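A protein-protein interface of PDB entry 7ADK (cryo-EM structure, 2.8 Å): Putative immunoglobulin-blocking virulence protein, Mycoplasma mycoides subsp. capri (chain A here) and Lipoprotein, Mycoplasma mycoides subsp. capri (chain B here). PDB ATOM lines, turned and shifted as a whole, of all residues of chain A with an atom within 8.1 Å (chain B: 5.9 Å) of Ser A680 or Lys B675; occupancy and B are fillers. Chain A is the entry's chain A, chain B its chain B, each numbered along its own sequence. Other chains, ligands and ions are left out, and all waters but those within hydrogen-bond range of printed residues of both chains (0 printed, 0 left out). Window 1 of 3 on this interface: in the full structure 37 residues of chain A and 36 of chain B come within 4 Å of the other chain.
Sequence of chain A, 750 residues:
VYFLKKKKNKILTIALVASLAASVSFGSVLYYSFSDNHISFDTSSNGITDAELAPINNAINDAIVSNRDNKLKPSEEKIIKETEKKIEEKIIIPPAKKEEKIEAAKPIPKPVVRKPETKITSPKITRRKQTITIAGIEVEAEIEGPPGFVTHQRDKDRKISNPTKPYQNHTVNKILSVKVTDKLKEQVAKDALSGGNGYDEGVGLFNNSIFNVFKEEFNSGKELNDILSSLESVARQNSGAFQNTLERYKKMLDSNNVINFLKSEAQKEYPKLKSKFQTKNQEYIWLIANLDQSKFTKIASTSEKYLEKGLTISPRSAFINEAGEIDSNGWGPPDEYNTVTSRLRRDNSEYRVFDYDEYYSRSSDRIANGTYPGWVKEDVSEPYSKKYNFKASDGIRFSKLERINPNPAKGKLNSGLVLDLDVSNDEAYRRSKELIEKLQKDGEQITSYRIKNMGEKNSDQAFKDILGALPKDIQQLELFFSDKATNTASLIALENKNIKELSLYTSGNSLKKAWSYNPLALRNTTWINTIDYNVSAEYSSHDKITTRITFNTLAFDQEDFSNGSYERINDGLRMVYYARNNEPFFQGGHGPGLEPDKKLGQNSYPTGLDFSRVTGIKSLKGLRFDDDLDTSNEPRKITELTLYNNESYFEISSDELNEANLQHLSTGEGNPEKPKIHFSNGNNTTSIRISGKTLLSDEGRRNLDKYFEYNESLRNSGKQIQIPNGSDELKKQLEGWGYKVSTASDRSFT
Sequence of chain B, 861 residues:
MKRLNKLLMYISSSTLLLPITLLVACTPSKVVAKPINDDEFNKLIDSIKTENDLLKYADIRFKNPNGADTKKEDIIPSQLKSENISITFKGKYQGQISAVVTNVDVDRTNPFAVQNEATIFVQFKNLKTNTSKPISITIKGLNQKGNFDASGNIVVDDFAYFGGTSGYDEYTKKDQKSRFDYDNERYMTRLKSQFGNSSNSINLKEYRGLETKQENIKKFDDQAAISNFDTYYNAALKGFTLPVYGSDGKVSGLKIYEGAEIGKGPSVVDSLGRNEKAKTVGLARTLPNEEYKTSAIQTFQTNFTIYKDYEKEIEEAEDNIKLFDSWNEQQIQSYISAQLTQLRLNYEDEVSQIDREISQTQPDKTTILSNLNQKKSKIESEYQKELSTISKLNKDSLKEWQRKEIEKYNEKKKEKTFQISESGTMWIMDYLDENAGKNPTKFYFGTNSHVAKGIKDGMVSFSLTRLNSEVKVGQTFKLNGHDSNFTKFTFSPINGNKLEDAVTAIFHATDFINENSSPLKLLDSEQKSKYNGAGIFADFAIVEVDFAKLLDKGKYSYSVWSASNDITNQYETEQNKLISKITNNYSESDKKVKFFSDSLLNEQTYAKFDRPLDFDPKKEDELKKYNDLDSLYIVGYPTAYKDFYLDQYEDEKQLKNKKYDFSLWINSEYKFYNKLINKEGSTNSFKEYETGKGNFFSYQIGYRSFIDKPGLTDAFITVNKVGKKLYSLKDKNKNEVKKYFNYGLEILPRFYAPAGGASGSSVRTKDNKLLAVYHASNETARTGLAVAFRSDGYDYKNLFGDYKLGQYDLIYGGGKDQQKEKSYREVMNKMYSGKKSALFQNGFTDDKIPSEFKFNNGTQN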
ATOM      1  N   ASP A 610       9.240 -15.316  -4.602  1.00  0.00           N
ATOM      2  CA  ASP A 610       7.859 -15.779  -4.723  1.00  0.00           C
ATOM      3  C   ASP A 610       7.635 -17.081  -3.932  1.00  0.00           C
ATOM      4  O   ASP A 610       8.265 -18.107  -4.183  1.00  0.00           O
ATOM      5  CB  ASP A 610       7.505 -15.916  -6.209  1.00  0.00           C
ATOM      6  CG  ASP A 610       6.122 -16.527  -6.441  1.00  0.00           C
ATOM      7  OD1 ASP A 610       5.207 -16.254  -5.642  1.00  0.00           O
ATOM      8  OD2 ASP A 610       5.947 -17.322  -7.387  1.00  0.00           O
ATOM      9  N   PHE A 611       6.696 -17.043  -2.993  1.00  0.00           N
ATOM     10  CA  PHE A 611       6.248 -18.181  -2.208  1.00  0.00           C
ATOM     11  C   PHE A 611       4.789 -18.569  -2.484  1.00  0.00           C
ATOM     12  O   PHE A 611       4.207 -19.332  -1.731  1.00  0.00           O
ATOM     13  CB  PHE A 611       6.553 -17.928  -0.730  1.00  0.00           C
ATOM     14  CG  PHE A 611       8.026 -17.782  -0.402  1.00  0.00           C
ATOM     15  CD1 PHE A 611       8.896 -18.867  -0.597  1.00  0.00           C
ATOM     16  CD2 PHE A 611       8.526 -16.594   0.147  1.00  0.00           C
ATOM     17  CE1 PHE A 611      10.242 -18.782  -0.217  1.00  0.00           C
ATOM     18  CE2 PHE A 611       9.877 -16.502   0.522  1.00  0.00           C
ATOM     19  CZ  PHE A 611      10.736 -17.598   0.339  1.00  0.00           C
ATOM     20  N   SER A 612       4.179 -18.119  -3.580  1.00  0.00           N
ATOM     21  CA  SER A 612       2.790 -18.430  -3.955  1.00  0.00           C
ATOM     22  C   SER A 612       2.454 -19.921  -4.078  1.00  0.00           C
ATOM     23  O   SER A 612       1.320 -20.323  -3.840  1.00  0.00           O
ATOM     24  CB  SER A 612       2.460 -17.793  -5.296  1.00  0.00           C
ATOM     25  OG  SER A 612       2.680 -16.411  -5.243  1.00  0.00           O
ATOM     26  N   ARG A 613       3.416 -20.770  -4.448  1.00  0.00           N
ATOM     27  CA  ARG A 613       3.198 -22.221  -4.550  1.00  0.00           C
ATOM     28  C   ARG A 613       3.375 -22.948  -3.217  1.00  0.00           C
ATOM     29  O   ARG A 613       2.977 -24.098  -3.132  1.00  0.00           O
ATOM     30  CB  ARG A 613       4.122 -22.832  -5.607  1.00  0.00           C
ATOM     31  CG  ARG A 613       3.942 -22.274  -7.019  1.00  0.00           C
ATOM     32  CD  ARG A 613       5.017 -22.848  -7.927  1.00  0.00           C
ATOM     33  NE  ARG A 613       5.025 -22.231  -9.253  1.00  0.00           N
ATOM     34  CZ  ARG A 613       6.032 -22.188 -10.099  1.00  0.00           C
ATOM     35  NH1 ARG A 613       7.185 -22.704  -9.834  1.00  0.00           N
ATOM     36  NH2 ARG A 613       5.904 -21.611 -11.238  1.00  0.00           N
ATOM     37  N   VAL A 614       3.952 -22.323  -2.186  1.00  0.00           N
ATOM     38  CA  VAL A 614       4.363 -22.980  -0.936  1.00  0.00           C
ATOM     39  C   VAL A 614       3.660 -22.346   0.257  1.00  0.00           C
ATOM     40  O   VAL A 614       4.072 -21.330   0.811  1.00  0.00           O
ATOM     41  CB  VAL A 614       5.895 -23.083  -0.836  1.00  0.00           C
ATOM     42  CG1 VAL A 614       6.669 -21.794  -1.091  1.00  0.00           C
ATOM     43  CG2 VAL A 614       6.358 -23.658   0.492  1.00  0.00           C
ATOM     44  N   THR A 615       2.537 -22.946   0.641  1.00  0.00           N
ATOM     45  CA  THR A 615       1.468 -22.267   1.392  1.00  0.00           C
ATOM     46  C   THR A 615       1.767 -22.018   2.872  1.00  0.00           C
ATOM     47  O   THR A 615       1.068 -21.230   3.506  1.00  0.00           O
ATOM     48  CB  THR A 615       0.130 -23.014   1.258  1.00  0.00           C
ATOM     49  OG1 THR A 615       0.170 -24.268   1.898  1.00  0.00           O
ATOM     50  CG2 THR A 615      -0.254 -23.253  -0.198  1.00  0.00           C
ATOM     51  N   LEU A 641       8.411  -9.440  -2.357  1.00  0.00           N
ATOM     52  CA  LEU A 641       8.034 -10.660  -1.659  1.00  0.00           C
ATOM     53  C   LEU A 641       6.587 -11.021  -1.971  1.00  0.00           C
ATOM     54  O   LEU A 641       5.679 -10.351  -1.512  1.00  0.00           O
ATOM     55  CB  LEU A 641       8.238 -10.429  -0.153  1.00  0.00           C
ATOM     56  CG  LEU A 641       7.815 -11.604   0.741  1.00  0.00           C
ATOM     57  CD1 LEU A 641       8.712 -12.816   0.539  1.00  0.00           C
ATOM     58  CD2 LEU A 641       7.841 -11.190   2.202  1.00  0.00           C
ATOM     59  N   THR A 642       6.358 -12.103  -2.696  1.00  0.00           N
ATOM     60  CA  THR A 642       5.011 -12.641  -2.913  1.00  0.00           C
ATOM     61  C   THR A 642       4.766 -13.819  -1.977  1.00  0.00           C
ATOM     62  O   THR A 642       5.600 -14.704  -1.844  1.00  0.00           O
ATOM     63  CB  THR A 642       4.751 -13.014  -4.376  1.00  0.00           C
ATOM     64  OG1 THR A 642       5.107 -11.966  -5.242  1.00  0.00           O
ATOM     65  CG2 THR A 642       3.275 -13.303  -4.604  1.00  0.00           C
ATOM     66  N   LEU A 643       3.619 -13.808  -1.310  1.00  0.00           N
ATOM     67  CA  LEU A 643       3.169 -14.771  -0.329  1.00  0.00           C
ATOM     68  C   LEU A 643       1.876 -15.430  -0.797  1.00  0.00           C
ATOM     69  O   LEU A 643       1.013 -14.802  -1.403  1.00  0.00           O
ATOM     70  CB  LEU A 643       2.971 -14.046   1.009  1.00  0.00           C
ATOM     71  CG  LEU A 643       4.244 -13.477   1.640  1.00  0.00           C
ATOM     72  CD1 LEU A 643       3.910 -12.645   2.862  1.00  0.00           C
ATOM     73  CD2 LEU A 643       5.212 -14.577   2.030  1.00  0.00           C
ATOM     74  N   TYR A 644       1.694 -16.690  -0.455  1.00  0.00           N
ATOM     75  CA  TYR A 644       0.396 -17.319  -0.573  1.00  0.00           C
ATOM     76  C   TYR A 644      -0.615 -16.712   0.399  1.00  0.00           C
ATOM     77  O   TYR A 644      -0.332 -16.598   1.593  1.00  0.00           O
ATOM     78  CB  TYR A 644       0.530 -18.811  -0.366  1.00  0.00           C
ATOM     79  CG  TYR A 644      -0.790 -19.520  -0.482  1.00  0.00           C
ATOM     80  CD1 TYR A 644      -1.366 -19.707  -1.745  1.00  0.00           C
ATOM     81  CD2 TYR A 644      -1.459 -19.955   0.672  1.00  0.00           C
ATOM     82  CE1 TYR A 644      -2.589 -20.370  -1.859  1.00  0.00           C
ATOM     83  CE2 TYR A 644      -2.674 -20.636   0.557  1.00  0.00           C
ATOM     84  CZ  TYR A 644      -3.229 -20.860  -0.712  1.00  0.00           C
ATOM     85  OH  TYR A 644      -4.356 -21.582  -0.848  1.00  0.00           O
ATOM     86  N   ASN A 645      -1.817 -16.380  -0.088  1.00  0.00           N
ATOM     87  CA  ASN A 645      -2.987 -16.188   0.763  1.00  0.00           C
ATOM     88  C   ASN A 645      -4.295 -16.617   0.089  1.00  0.00           C
ATOM     89  O   ASN A 645      -4.430 -16.568  -1.126  1.00  0.00           O
ATOM     90  CB  ASN A 645      -3.063 -14.753   1.295  1.00  0.00           C
ATOM     91  CG  ASN A 645      -3.919 -14.682   2.539  1.00  0.00           C
ATOM     92  OD1 ASN A 645      -4.099 -15.650   3.256  1.00  0.00           O
ATOM     93  ND2 ASN A 645      -4.511 -13.569   2.828  1.00  0.00           N
ATOM     94  N   ASN A 646      -5.245 -17.036   0.913  1.00  0.00           N
ATOM     95  CA  ASN A 646      -6.376 -17.900   0.584  1.00  0.00           C
ATOM     96  C   ASN A 646      -7.732 -17.263   0.943  1.00  0.00           C
ATOM     97  O   ASN A 646      -8.767 -17.591   0.367  1.00  0.00           O
ATOM     98  CB  ASN A 646      -6.115 -19.171   1.414  1.00  0.00           C
ATOM     99  CG  ASN A 646      -6.872 -20.411   0.995  1.00  0.00           C
ATOM    100  OD1 ASN A 646      -7.804 -20.396   0.229  1.00  0.00           O
ATOM    101  ND2 ASN A 646      -6.471 -21.549   1.476  1.00  0.00           N
ATOM    102  N   HIS A 678       3.305  -8.729  -1.882  1.00  0.00           N
ATOM    103  CA  HIS A 678       2.177  -9.185  -2.698  1.00  0.00           C
ATOM    104  C   HIS A 678       1.540 -10.441  -2.108  1.00  0.00           C
ATOM    105  O   HIS A 678       2.202 -11.204  -1.417  1.00  0.00           O
ATOM    106  CB  HIS A 678       2.642  -9.512  -4.114  1.00  0.00           C
ATOM    107  CG  HIS A 678       2.980  -8.349  -4.986  1.00  0.00           C
ATOM    108  ND1 HIS A 678       2.068  -7.577  -5.706  1.00  0.00           N
ATOM    109  CD2 HIS A 678       4.236  -7.976  -5.324  1.00  0.00           C
ATOM    110  CE1 HIS A 678       2.805  -6.753  -6.463  1.00  0.00           C
ATOM    111  NE2 HIS A 678       4.107  -6.972  -6.245  1.00  0.00           N
ATOM    112  N   PHE A 679       0.289 -10.720  -2.454  1.00  0.00           N
ATOM    113  CA  PHE A 679      -0.407 -11.951  -2.082  1.00  0.00           C
ATOM    114  C   PHE A 679      -1.054 -12.621  -3.292  1.00  0.00           C
ATOM    115  O   PHE A 679      -1.550 -11.936  -4.181  1.00  0.00           O
ATOM    116  CB  PHE A 679      -1.438 -11.661  -0.994  1.00  0.00           C
ATOM    117  CG  PHE A 679      -0.870 -11.186   0.320  1.00  0.00           C
ATOM    118  CD1 PHE A 679      -0.216 -12.097   1.153  1.00  0.00           C
ATOM    119  CD2 PHE A 679      -0.976  -9.843   0.714  1.00  0.00           C
ATOM    120  CE1 PHE A 679       0.343 -11.671   2.361  1.00  0.00           C
ATOM    121  CE2 PHE A 679      -0.408  -9.412   1.920  1.00  0.00           C
ATOM    122  CZ  PHE A 679       0.255 -10.327   2.745  1.00  0.00           C
ATOM    123  N   SER A 680      -1.115 -13.949  -3.320  1.00  0.00           N
ATOM    124  CA  SER A 680      -1.644 -14.716  -4.463  1.00  0.00           C
ATOM    125  C   SER A 680      -3.102 -14.424  -4.862  1.00  0.00           C
ATOM    126  O   SER A 680      -3.482 -14.647  -6.008  1.00  0.00           O
ATOM    127  CB  SER A 680      -1.503 -16.209  -4.175  1.00  0.00           C
ATOM    128  OG  SER A 680      -0.175 -16.538  -3.881  1.00  0.00           O
ATOM    129  N   ASN A 681      -3.917 -13.893  -3.954  1.00  0.00           N
ATOM    130  CA  ASN A 681      -5.322 -13.553  -4.165  1.00  0.00           C
ATOM    131  C   ASN A 681      -5.584 -12.081  -4.571  1.00  0.00           C
ATOM    132  O   ASN A 681      -6.398 -11.821  -5.452  1.00  0.00           O
ATOM    133  CB  ASN A 681      -6.098 -13.946  -2.892  1.00  0.00           C
ATOM    134  CG  ASN A 681      -5.642 -13.227  -1.644  1.00  0.00           C
ATOM    135  OD1 ASN A 681      -4.544 -12.708  -1.567  1.00  0.00           O
ATOM    136  ND2 ASN A 681      -6.476 -13.102  -0.654  1.00  0.00           N
ATOM    137  N   GLY A 682      -4.959 -11.102  -3.907  1.00  0.00           N
ATOM    138  CA  GLY A 682      -5.307  -9.670  -3.961  1.00  0.00           C
ATOM    139  C   GLY A 682      -6.594  -9.200  -3.236  1.00  0.00           C
ATOM    140  O   GLY A 682      -6.816  -8.000  -3.117  1.00  0.00           O
ATOM    141  N   ASN A 683      -7.417 -10.105  -2.681  1.00  0.00           N
ATOM    142  CA  ASN A 683      -8.629  -9.830  -1.883  1.00  0.00           C
ATOM    143  C   ASN A 683      -8.370  -9.347  -0.443  1.00  0.00           C
ATOM    144  O   ASN A 683      -9.299  -9.294   0.356  1.00  0.00           O
ATOM    145  CB  ASN A 683      -9.552 -11.075  -1.870  1.00  0.00           C
ATOM    146  CG  ASN A 683     -10.158 -11.402  -3.221  1.00  0.00           C
ATOM    147  OD1 ASN A 683      -9.456 -11.599  -4.193  1.00  0.00           O
ATOM    148  ND2 ASN A 683     -11.458 -11.413  -3.344  1.00  0.00           N
ATOM    149  N   ASN A 684      -7.138  -9.000  -0.087  1.00  0.00           N
ATOM    150  CA  ASN A 684      -6.688  -8.730   1.287  1.00  0.00           C
ATOM    151  C   ASN A 684      -7.099  -7.362   1.858  1.00  0.00           C
ATOM    152  O   ASN A 684      -6.353  -6.729   2.601  1.00  0.00           O
ATOM    153  CB  ASN A 684      -5.184  -8.964   1.401  1.00  0.00           C
ATOM    154  CG  ASN A 684      -4.807 -10.253   0.747  1.00  0.00           C
ATOM    155  OD1 ASN A 684      -5.027 -11.327   1.264  1.00  0.00           O
ATOM    156  ND2 ASN A 684      -4.320 -10.194  -0.458  1.00  0.00           N
ATOM    157  N   ASN A 711       2.421  -3.330   1.001  1.00  0.00           N
ATOM    158  CA  ASN A 711       1.338  -3.976   0.263  1.00  0.00           C
ATOM    159  C   ASN A 711       0.190  -2.998   0.029  1.00  0.00           C
ATOM    160  O   ASN A 711      -0.484  -2.617   0.981  1.00  0.00           O
ATOM    161  CB  ASN A 711       0.877  -5.208   1.034  1.00  0.00           C
ATOM    162  CG  ASN A 711      -0.202  -5.967   0.316  1.00  0.00           C
ATOM    163  OD1 ASN A 711       0.033  -6.812  -0.516  1.00  0.00           O
ATOM    164  ND2 ASN A 711      -1.435  -5.697   0.610  1.00  0.00           N
ATOM    165  N   THR B 476      -6.157 -16.996 -18.764  1.00  0.00           N
ATOM    166  CA  THR B 476      -6.228 -15.574 -19.144  1.00  0.00           C
ATOM    167  C   THR B 476      -5.616 -15.354 -20.528  1.00  0.00           C
ATOM    168  O   THR B 476      -4.463 -15.707 -20.773  1.00  0.00           O
ATOM    169  CB  THR B 476      -5.593 -14.679 -18.074  1.00  0.00           C
ATOM    170  OG1 THR B 476      -6.385 -14.755 -16.921  1.00  0.00           O
ATOM    171  CG2 THR B 476      -5.553 -13.201 -18.427  1.00  0.00           C
ATOM    172  N   LYS B 671     -10.301  -8.672  -9.259  1.00  0.00           N
ATOM    173  CA  LYS B 671      -9.277  -9.414  -8.518  1.00  0.00           C
ATOM    174  C   LYS B 671      -8.839 -10.714  -9.181  1.00  0.00           C
ATOM    175  O   LYS B 671      -7.785 -11.225  -8.830  1.00  0.00           O
ATOM    176  CB  LYS B 671      -9.796  -9.679  -7.096  1.00  0.00           C
ATOM    177  CG  LYS B 671      -9.932  -8.366  -6.312  1.00  0.00           C
ATOM    178  CD  LYS B 671     -10.554  -8.560  -4.931  1.00  0.00           C
ATOM    179  CE  LYS B 671     -10.649  -7.206  -4.220  1.00  0.00           C
ATOM    180  NZ  LYS B 671     -11.486  -7.270  -3.007  1.00  0.00           N
ATOM    181  N   PHE B 672      -9.582 -11.242 -10.149  1.00  0.00           N
ATOM    182  CA  PHE B 672      -9.273 -12.514 -10.809  1.00  0.00           C
ATOM    183  C   PHE B 672      -8.178 -12.444 -11.887  1.00  0.00           C
ATOM    184  O   PHE B 672      -7.723 -13.494 -12.328  1.00  0.00           O
ATOM    185  CB  PHE B 672     -10.563 -13.073 -11.427  1.00  0.00           C
ATOM    186  CG  PHE B 672     -11.674 -13.548 -10.501  1.00  0.00           C
ATOM    187  CD1 PHE B 672     -11.461 -13.791  -9.133  1.00  0.00           C
ATOM    188  CD2 PHE B 672     -12.944 -13.799 -11.053  1.00  0.00           C
ATOM    189  CE1 PHE B 672     -12.514 -14.241  -8.325  1.00  0.00           C
ATOM    190  CE2 PHE B 672     -14.003 -14.238 -10.242  1.00  0.00           C
ATOM    191  CZ  PHE B 672     -13.789 -14.447  -8.875  1.00  0.00           C
ATOM    192  N   TYR B 673      -7.731 -11.260 -12.327  1.00  0.00           N
ATOM    193  CA  TYR B 673      -7.173 -11.057 -13.674  1.00  0.00           C
ATOM    194  C   TYR B 673      -6.062 -12.011 -14.148  1.00  0.00           C
ATOM    195  O   TYR B 673      -6.218 -12.668 -15.174  1.00  0.00           O
ATOM    196  CB  TYR B 673      -6.740  -9.594 -13.847  1.00  0.00           C
ATOM    197  CG  TYR B 673      -6.262  -9.278 -15.257  1.00  0.00           C
ATOM    198  CD1 TYR B 673      -7.112  -9.544 -16.341  1.00  0.00           C
ATOM    199  CD2 TYR B 673      -4.969  -8.777 -15.503  1.00  0.00           C
ATOM    200  CE1 TYR B 673      -6.673  -9.349 -17.654  1.00  0.00           C
ATOM    201  CE2 TYR B 673      -4.527  -8.583 -16.828  1.00  0.00           C
ATOM    202  CZ  TYR B 673      -5.382  -8.870 -17.908  1.00  0.00           C
ATOM    203  OH  TYR B 673      -5.002  -8.641 -19.192  1.00  0.00           O
ATOM    204  N   ASN B 674      -4.951 -12.108 -13.423  1.00  0.00           N
ATOM    205  CA  ASN B 674      -3.835 -13.014 -13.731  1.00  0.00           C
ATOM    206  C   ASN B 674      -3.677 -14.106 -12.654  1.00  0.00           C
ATOM    207  O   ASN B 674      -2.593 -14.650 -12.448  1.00  0.00           O
ATOM    208  CB  ASN B 674      -2.561 -12.169 -13.976  1.00  0.00           C
ATOM    209  CG  ASN B 674      -2.304 -11.854 -15.436  1.00  0.00           C
ATOM    210  OD1 ASN B 674      -2.501 -12.660 -16.325  1.00  0.00           O
ATOM    211  ND2 ASN B 674      -1.771 -10.695 -15.733  1.00  0.00           N
ATOM    212  N   LYS B 675      -4.751 -14.395 -11.908  1.00  0.00           N
ATOM    213  CA  LYS B 675      -4.686 -15.084 -10.613  1.00  0.00           C
ATOM    214  C   LYS B 675      -5.335 -16.474 -10.599  1.00  0.00           C
ATOM    215  O   LYS B 675      -5.064 -17.255  -9.695  1.00  0.00           O
ATOM    216  CB  LYS B 675      -5.268 -14.150  -9.540  1.00  0.00           C
ATOM    217  CG  LYS B 675      -4.613 -12.765  -9.413  1.00  0.00           C
ATOM    218  CD  LYS B 675      -3.171 -12.829  -8.898  1.00  0.00           C
ATOM    219  CE  LYS B 675      -2.656 -11.425  -8.566  1.00  0.00           C
ATOM    220  NZ  LYS B 675      -1.346 -11.457  -7.886  1.00  0.00           N
ATOM    221  N   LEU B 676      -6.164 -16.803 -11.591  1.00  0.00           N
ATOM    222  CA  LEU B 676      -6.899 -18.076 -11.720  1.00  0.00           C
ATOM    223  C   LEU B 676      -6.095 -19.202 -12.409  1.00  0.00           C
ATOM    224  O   LEU B 676      -6.616 -20.299 -12.565  1.00  0.00           O
ATOM    225  CB  LEU B 676      -8.234 -17.797 -12.456  1.00  0.00           C
ATOM    226  CG  LEU B 676      -9.443 -17.497 -11.556  1.00  0.00           C
ATOM    227  CD1 LEU B 676      -9.176 -16.428 -10.508  1.00  0.00           C
ATOM    228  CD2 LEU B 676     -10.616 -17.040 -12.411  1.00  0.00           C
ATOM    229  N   ILE B 677      -4.846 -18.966 -12.826  1.00  0.00           N
ATOM    230  CA  ILE B 677      -4.056 -19.934 -13.607  1.00  0.00           C
ATOM    231  C   ILE B 677      -3.739 -21.192 -12.768  1.00  0.00           C
ATOM    232  O   ILE B 677      -2.971 -21.150 -11.806  1.00  0.00           O
ATOM    233  CB  ILE B 677      -2.763 -19.283 -14.175  1.00  0.00           C
ATOM    234  CG1 ILE B 677      -2.926 -17.870 -14.786  1.00  0.00           C
ATOM    235  CG2 ILE B 677      -2.114 -20.223 -15.205  1.00  0.00           C
ATOM    236  CD1 ILE B 677      -3.871 -17.739 -15.977  1.00  0.00           C
ATOM    237  N   SER B 685      -5.986 -20.232  -5.116  1.00  0.00           N
ATOM    238  CA  SER B 685      -5.884 -19.063  -4.239  1.00  0.00           C
ATOM    239  C   SER B 685      -7.241 -18.428  -3.891  1.00  0.00           C
ATOM    240  O   SER B 685      -7.296 -17.509  -3.076  1.00  0.00           O
ATOM    241  CB  SER B 685      -4.948 -18.052  -4.903  1.00  0.00           C
ATOM    242  OG  SER B 685      -4.488 -17.101  -3.970  1.00  0.00           O
ATOM    243  N   PHE B 686      -8.340 -18.905  -4.484  1.00  0.00           N
ATOM    244  CA  PHE B 686      -9.712 -18.449  -4.240  1.00  0.00           C
ATOM    245  C   PHE B 686     -10.627 -19.629  -3.896  1.00  0.00           C
ATOM    246  O   PHE B 686     -10.468 -20.724  -4.440  1.00  0.00           O
ATOM    247  CB  PHE B 686     -10.240 -17.684  -5.458  1.00  0.00           C
ATOM    248  CG  PHE B 686      -9.377 -16.515  -5.865  1.00  0.00           C
ATOM    249  CD1 PHE B 686      -9.530 -15.259  -5.251  1.00  0.00           C
ATOM    250  CD2 PHE B 686      -8.384 -16.700  -6.835  1.00  0.00           C
ATOM    251  CE1 PHE B 686      -8.692 -14.190  -5.612  1.00  0.00           C
ATOM    252  CE2 PHE B 686      -7.542 -15.640  -7.186  1.00  0.00           C
ATOM    253  CZ  PHE B 686      -7.694 -14.381  -6.580  1.00  0.00           C
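The backbone carbonyl oxygen of Ser A680 sits close to the side-chain hydroxyl of Ser B685 (3.3 Å). The side-chain hydroxyl (OG) of Ser B685 lies within hydrogen-bond range of the backbone NH (N) of Asn A681, at 3.3 Å. O of Asn A645 is in hydrogen-bond range of OG of Ser B685, 2.9 Å away.
The side-chain hydroxyl (OG) of Ser A680 lies within hydrogen-bond range of the side-chain hydroxyl (OG) of Ser A612 (3.2 Å). OD1 of Asn A681 sits at hydrogen-bond distance from ND2 of Asn A684, at 2.8 Å. The backbone carbonyl oxygen (O) of Asn A681 sits close to the side-chain amide oxygen (OD1) of Asn A683 (3.3 Å). O of Leu A643 is in hydrogen-bond range of N of Ser A680. OD1 of Asn A684 lies within hydrogen-bond range of ND2 of Asn A645 (2.8 Å). ND2 of Asn A646 lies within hydrogen-bond range of OH of Tyr A644, at 3.1 Å.
Among the printed residues, merely in contact across the chains: Asn A646 with Ser B685 (3.7 Å), Phe A679 with Lys B675 (3.7 Å), Ser A680 with Lys B675 (3.4 Å), Asn A681 with Lys B671 (3.7 Å), Asn A681 with Phe B686 (3.1 Å), Asn A683 with Lys B671 (3.3 Å) and Asn A683 with Phe B686 (3.1 Å).
Among the printed residues, 10 pairs touch across the chains. Among the printed residues, no Asp or Glu carboxylate lies within 4 Å of a Lys or Arg side-chain nitrogen of the other chain.
Of the printed residues of chain B, Ser A680 touches Lys B675 and Ser B685. Of the printed residues of chain A, Lys B675 touches Phe A679 and Ser A680. Of the printed residues of chain A, Lys B671 touches Asn A681 and Asn A683. Printed residues of chain A within 4 Å of Phe B686: Asn A681 and Asn A683. Of the printed residues of chain B, Phe A679 touches Lys B675. Of the printed residues of chain B, Asn A683 touches Lys B671 and Phe B686. Leu B676 touches none of the printed residues of chain A. Phe A611 touches none of the printed residues of chain B. The nearest residue of chain A that does not touch Lys B675 is Asn A681 (4.4 Å). The nearest printed residue of chain B that does not touch Phe A679 is Ser B685 (5.7 Å).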
